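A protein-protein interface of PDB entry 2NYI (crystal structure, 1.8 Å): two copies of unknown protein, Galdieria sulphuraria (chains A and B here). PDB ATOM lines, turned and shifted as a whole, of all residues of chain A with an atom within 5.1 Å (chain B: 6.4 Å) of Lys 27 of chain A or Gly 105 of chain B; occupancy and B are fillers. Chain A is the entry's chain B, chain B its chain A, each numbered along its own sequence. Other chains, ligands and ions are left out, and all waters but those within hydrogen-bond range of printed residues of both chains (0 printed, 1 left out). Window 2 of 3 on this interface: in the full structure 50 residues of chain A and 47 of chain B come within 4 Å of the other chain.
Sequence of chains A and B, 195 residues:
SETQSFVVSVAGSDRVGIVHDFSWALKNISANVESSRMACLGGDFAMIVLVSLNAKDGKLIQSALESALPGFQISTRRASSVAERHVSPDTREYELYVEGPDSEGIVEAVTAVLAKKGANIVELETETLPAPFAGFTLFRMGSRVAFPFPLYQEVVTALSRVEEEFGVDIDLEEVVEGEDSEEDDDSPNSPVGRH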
ATOM      1  N   SER A  23      -1.736   3.956 -34.164  1.00  0.00           N
ATOM      2  CA  SER A  23      -1.616   3.230 -32.892  1.00  0.00           C
ATOM      3  C   SER A  23      -1.857   1.724 -33.038  1.00  0.00           C
ATOM      4  O   SER A  23      -1.224   0.918 -32.348  1.00  0.00           O
ATOM      5  CB  SER A  23      -2.538   3.834 -31.842  1.00  0.00           C
ATOM      6  OG  SER A  23      -3.885   3.722 -32.231  1.00  0.00           O
ATOM      7  N   TRP A  24      -2.758   1.346 -33.943  1.00  0.00           N
ATOM      8  CA  TRP A  24      -2.937  -0.074 -34.270  1.00  0.00           C
ATOM      9  C   TRP A  24      -1.633  -0.639 -34.853  1.00  0.00           C
ATOM     10  O   TRP A  24      -1.189  -1.711 -34.457  1.00  0.00           O
ATOM     11  CB  TRP A  24      -4.139  -0.311 -35.208  1.00  0.00           C
ATOM     12  CG  TRP A  24      -4.446  -1.783 -35.290  1.00  0.00           C
ATOM     13  CD1 TRP A  24      -5.375  -2.470 -34.556  1.00  0.00           C
ATOM     14  CD2 TRP A  24      -3.757  -2.756 -36.080  1.00  0.00           C
ATOM     15  NE1 TRP A  24      -5.318  -3.813 -34.862  1.00  0.00           N
ATOM     16  CE2 TRP A  24      -4.338  -4.013 -35.799  1.00  0.00           C
ATOM     17  CE3 TRP A  24      -2.717  -2.688 -37.016  1.00  0.00           C
ATOM     18  CZ2 TRP A  24      -3.901  -5.203 -36.412  1.00  0.00           C
ATOM     19  CZ3 TRP A  24      -2.280  -3.882 -37.637  1.00  0.00           C
ATOM     20  CH2 TRP A  24      -2.880  -5.117 -37.327  1.00  0.00           C
ATOM     21  N   ALA A  25      -1.027   0.078 -35.796  1.00  0.00           N
ATOM     22  CA  ALA A  25       0.233  -0.373 -36.390  1.00  0.00           C
ATOM     23  C   ALA A  25       1.325  -0.622 -35.339  1.00  0.00           C
ATOM     24  O   ALA A  25       1.982  -1.666 -35.369  1.00  0.00           O
ATOM     25  CB  ALA A  25       0.706   0.601 -37.481  1.00  0.00           C
ATOM     26  N   LEU A  26       1.485   0.308 -34.398  1.00  0.00           N
ATOM     27  CA  LEU A  26       2.430   0.169 -33.289  1.00  0.00           C
ATOM     28  C   LEU A  26       2.088  -1.013 -32.383  1.00  0.00           C
ATOM     29  O   LEU A  26       2.952  -1.808 -32.026  1.00  0.00           O
ATOM     30  CB  LEU A  26       2.490   1.458 -32.468  1.00  0.00           C
ATOM     31  CG  LEU A  26       3.101   2.675 -33.182  1.00  0.00           C
ATOM     32  CD1 LEU A  26       3.367   3.715 -32.119  1.00  0.00           C
ATOM     33  CD2 LEU A  26       4.411   2.320 -33.889  1.00  0.00           C
ATOM     34  N   LYS A  27       0.823  -1.138 -32.018  1.00  0.00           N
ATOM     35  CA  LYS A  27       0.407  -2.242 -31.151  1.00  0.00           C
ATOM     36  C   LYS A  27       0.732  -3.591 -31.806  1.00  0.00           C
ATOM     37  O   LYS A  27       1.216  -4.520 -31.138  1.00  0.00           O
ATOM     38  CB  LYS A  27      -1.087  -2.129 -30.822  1.00  0.00           C
ATOM     39  CG  LYS A  27      -1.557  -3.143 -29.783  1.00  0.00           C
ATOM     40  CD  LYS A  27      -3.054  -3.027 -29.534  1.00  0.00           C
ATOM     41  CE  LYS A  27      -3.511  -3.949 -28.389  1.00  0.00           C
ATOM     42  NZ  LYS A  27      -3.405  -5.384 -28.749  1.00  0.00           N
ATOM     43  N   ASN A  28       0.514  -3.678 -33.117  1.00  0.00           N
ATOM     44  CA  ASN A  28       0.776  -4.886 -33.882  1.00  0.00           C
ATOM     45  C   ASN A  28       2.258  -5.304 -33.905  1.00  0.00           C
ATOM     46  O   ASN A  28       2.576  -6.496 -34.049  1.00  0.00           O
ATOM     47  CB  ASN A  28       0.245  -4.717 -35.306  1.00  0.00           C
ATOM     48  CG  ASN A  28       0.482  -5.927 -36.164  1.00  0.00           C
ATOM     49  OD1 ASN A  28      -0.140  -6.972 -35.951  1.00  0.00           O
ATOM     50  ND2 ASN A  28       1.392  -5.804 -37.134  1.00  0.00           N
ATOM     51  N   ILE A  29       3.158  -4.339 -33.760  1.00  0.00           N
ATOM     52  CA  ILE A  29       4.587  -4.692 -33.697  1.00  0.00           C
ATOM     53  C   ILE A  29       5.128  -4.651 -32.259  1.00  0.00           C
ATOM     54  O   ILE A  29       6.349  -4.673 -32.063  1.00  0.00           O
ATOM     55  CB  ILE A  29       5.468  -3.820 -34.631  1.00  0.00           C
ATOM     56  CG1 ILE A  29       5.370  -2.323 -34.263  1.00  0.00           C
ATOM     57  CG2 ILE A  29       5.121  -4.104 -36.124  1.00  0.00           C
ATOM     58  CD1 ILE A  29       6.385  -1.440 -34.988  1.00  0.00           C
ATOM     59  N   SER A  30       4.217  -4.593 -31.285  1.00  0.00           N
ATOM     60  CA  SER A  30       4.538  -4.572 -29.846  1.00  0.00           C
ATOM     61  C   SER A  30       5.332  -3.343 -29.408  1.00  0.00           C
ATOM     62  O   SER A  30       6.118  -3.396 -28.445  1.00  0.00           O
ATOM     63  CB  SER A  30       5.263  -5.859 -29.423  1.00  0.00           C
ATOM     64  OG  SER A  30       4.386  -6.963 -29.475  1.00  0.00           O
ATOM     65  N   ALA A  31       5.115  -2.237 -30.108  1.00  0.00           N
ATOM     66  CA  ALA A  31       5.723  -0.956 -29.769  1.00  0.00           C
ATOM     67  C   ALA A  31       4.746  -0.210 -28.862  1.00  0.00           C
ATOM     68  O   ALA A  31       3.527  -0.332 -29.028  1.00  0.00           O
ATOM     69  CB  ALA A  31       6.004  -0.162 -31.041  1.00  0.00           C
ATOM     70  N   SER B 103      -0.657   0.660 -20.451  1.00  0.00           N
ATOM     71  CA  SER B 103      -0.697  -0.653 -21.067  1.00  0.00           C
ATOM     72  C   SER B 103      -0.508  -0.496 -22.576  1.00  0.00           C
ATOM     73  O   SER B 103      -0.681   0.603 -23.120  1.00  0.00           O
ATOM     74  CB  SER B 103      -2.022  -1.353 -20.751  1.00  0.00           C
ATOM     75  OG  SER B 103      -3.109  -0.748 -21.421  1.00  0.00           O
ATOM     76  N   GLU B 104      -0.134  -1.587 -23.246  1.00  0.00           N
ATOM     77  CA  GLU B 104       0.107  -1.579 -24.694  1.00  0.00           C
ATOM     78  C   GLU B 104      -1.128  -1.122 -25.493  1.00  0.00           C
ATOM     79  O   GLU B 104      -0.990  -0.485 -26.539  1.00  0.00           O
ATOM     80  CB  GLU B 104       0.561  -2.977 -25.162  1.00  0.00           C
ATOM     81  CG  GLU B 104       1.084  -3.075 -26.614  1.00  0.00           C
ATOM     82  CD  GLU B 104       1.396  -4.519 -27.059  1.00  0.00           C
ATOM     83  OE1 GLU B 104       1.834  -5.332 -26.211  1.00  0.00           O
ATOM     84  OE2 GLU B 104       1.219  -4.844 -28.264  1.00  0.00           O
ATOM     85  N   GLY B 105      -2.325  -1.421 -24.984  1.00  0.00           N
ATOM     86  CA  GLY B 105      -3.552  -1.239 -25.770  1.00  0.00           C
ATOM     87  C   GLY B 105      -4.458  -0.027 -25.560  1.00  0.00           C
ATOM     88  O   GLY B 105      -5.422   0.133 -26.305  1.00  0.00           O
ATOM     89  N   ILE B 106      -4.180   0.812 -24.558  1.00  0.00           N
ATOM     90  CA  ILE B 106      -5.086   1.935 -24.232  1.00  0.00           C
ATOM     91  C   ILE B 106      -5.324   2.876 -25.414  1.00  0.00           C
ATOM     92  O   ILE B 106      -6.464   3.111 -25.815  1.00  0.00           O
ATOM     93  CB  ILE B 106      -4.585   2.831 -23.078  1.00  0.00           C
ATOM     94  CG1 ILE B 106      -3.991   2.030 -21.942  1.00  0.00           C
ATOM     95  CG2 ILE B 106      -5.722   3.723 -22.574  1.00  0.00           C
ATOM     96  CD1 ILE B 106      -3.139   2.881 -21.040  1.00  0.00           C
ATOM     97  N   VAL B 107      -4.238   3.409 -25.964  1.00  0.00           N
ATOM     98  CA  VAL B 107      -4.331   4.368 -27.063  1.00  0.00           C
ATOM     99  C   VAL B 107      -5.120   3.789 -28.245  1.00  0.00           C
ATOM    100  O   VAL B 107      -6.055   4.426 -28.731  1.00  0.00           O
ATOM    101  CB  VAL B 107      -2.930   4.869 -27.498  1.00  0.00           C
ATOM    102  CG1 VAL B 107      -3.057   5.895 -28.596  1.00  0.00           C
ATOM    103  CG2 VAL B 107      -2.179   5.475 -26.291  1.00  0.00           C
ATOM    104  N   GLU B 108      -4.756   2.581 -28.700  1.00  0.00           N
ATOM    105  CA  GLU B 108      -5.508   1.934 -29.790  1.00  0.00           C
ATOM    106  C   GLU B 108      -6.976   1.776 -29.417  1.00  0.00           C
ATOM    107  O   GLU B 108      -7.863   2.023 -30.246  1.00  0.00           O
ATOM    108  CB  GLU B 108      -4.891   0.574 -30.176  1.00  0.00           C
ATOM    109  CG  GLU B 108      -5.456  -0.033 -31.481  1.00  0.00           C
ATOM    110  CD  GLU B 108      -6.807  -0.729 -31.312  1.00  0.00           C
ATOM    111  OE1 GLU B 108      -7.152  -1.170 -30.186  1.00  0.00           O
ATOM    112  OE2 GLU B 108      -7.527  -0.836 -32.319  1.00  0.00           O
ATOM    113  N   ALA B 109      -7.239   1.356 -28.180  1.00  0.00           N
ATOM    114  CA  ALA B 109      -8.623   1.121 -27.745  1.00  0.00           C
ATOM    115  C   ALA B 109      -9.485   2.393 -27.739  1.00  0.00           C
ATOM    116  O   ALA B 109     -10.624   2.362 -28.199  1.00  0.00           O
ATOM    117  CB  ALA B 109      -8.660   0.444 -26.374  1.00  0.00           C
ATOM    118  N   VAL B 110      -8.939   3.496 -27.211  1.00  0.00           N
ATOM    119  CA  VAL B 110      -9.680   4.760 -27.131  1.00  0.00           C
ATOM    120  C   VAL B 110      -9.911   5.295 -28.530  1.00  0.00           C
ATOM    121  O   VAL B 110     -11.042   5.622 -28.897  1.00  0.00           O
ATOM    122  CB  VAL B 110      -8.955   5.827 -26.268  1.00  0.00           C
ATOM    123  CG1 VAL B 110      -9.674   7.177 -26.344  1.00  0.00           C
ATOM    124  CG2 VAL B 110      -8.841   5.349 -24.811  1.00  0.00           C
ATOM    125  N   PHE B 166      -9.637  -1.898 -19.711  1.00  0.00           N
ATOM    126  CA  PHE B 166      -8.282  -1.390 -19.502  1.00  0.00           C
ATOM    127  C   PHE B 166      -8.011  -0.798 -18.117  1.00  0.00           C
ATOM    128  O   PHE B 166      -6.873  -0.437 -17.825  1.00  0.00           O
ATOM    129  CB  PHE B 166      -7.914  -0.397 -20.620  1.00  0.00           C
ATOM    130  CG  PHE B 166      -7.666  -1.073 -21.932  1.00  0.00           C
ATOM    131  CD1 PHE B 166      -6.405  -1.562 -22.242  1.00  0.00           C
ATOM    132  CD2 PHE B 166      -8.710  -1.294 -22.824  1.00  0.00           C
ATOM    133  CE1 PHE B 166      -6.166  -2.226 -23.441  1.00  0.00           C
ATOM    134  CE2 PHE B 166      -8.479  -1.967 -24.027  1.00  0.00           C
ATOM    135  CZ  PHE B 166      -7.205  -2.434 -24.332  1.00  0.00           C
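No position is printed for both chains.
Of the 6 pairs that touch across the chains among the printed residues, none has its exchanged pair printed and touching as well.
Printed residues of chain B within 4 Å of Trp 24 of chain A: Glu 108 (3.5 Å).
Lys 27 of chain A touches just these residues of chain B: Glu 104 and Gly 105.
Of the printed residues of chain B, Ser 30 of chain A touches Glu 104.
Ser 103 of chain B touches none of the printed residues of chain A.
Of the printed residues of chain A, Gly 105 of chain B touches Lys 27.
Ile 106 of chain B touches none of the printed residues of chain A.
Of the printed residues of chain A, Glu 108 of chain B touches Ser 23 (3.4 Å) and Trp 24 (3.5 Å).
The nearest residue of chain B that does not touch Lys 27 of chain A is Glu 108 of chain B (4.1 Å).
The nearest printed residue of chain A that does not touch Gly 105 of chain B is Ser 23 of chain A (7.1 Å).
The nearest printed residue of chain A that does not touch Val 107 of chain B is Trp 24 of chain A (6.6 Å).
OE2 of Glu 104 of chain B lies close to O of Lys 27 of chain A (2.9 Å).
Among the printed residues, 6 pairs touch across the chains.
Among the printed residues, merely in contact across the chains: Ser 23 of chain A with Val 107 of chain B, Ser 23 of chain A with Glu 108 of chain B, Trp 24 of chain A with Glu 108 of chain B, Lys 27 of chain A with Gly 105 of chain B and Ser 30 of chain A with Glu 104 of chain B.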
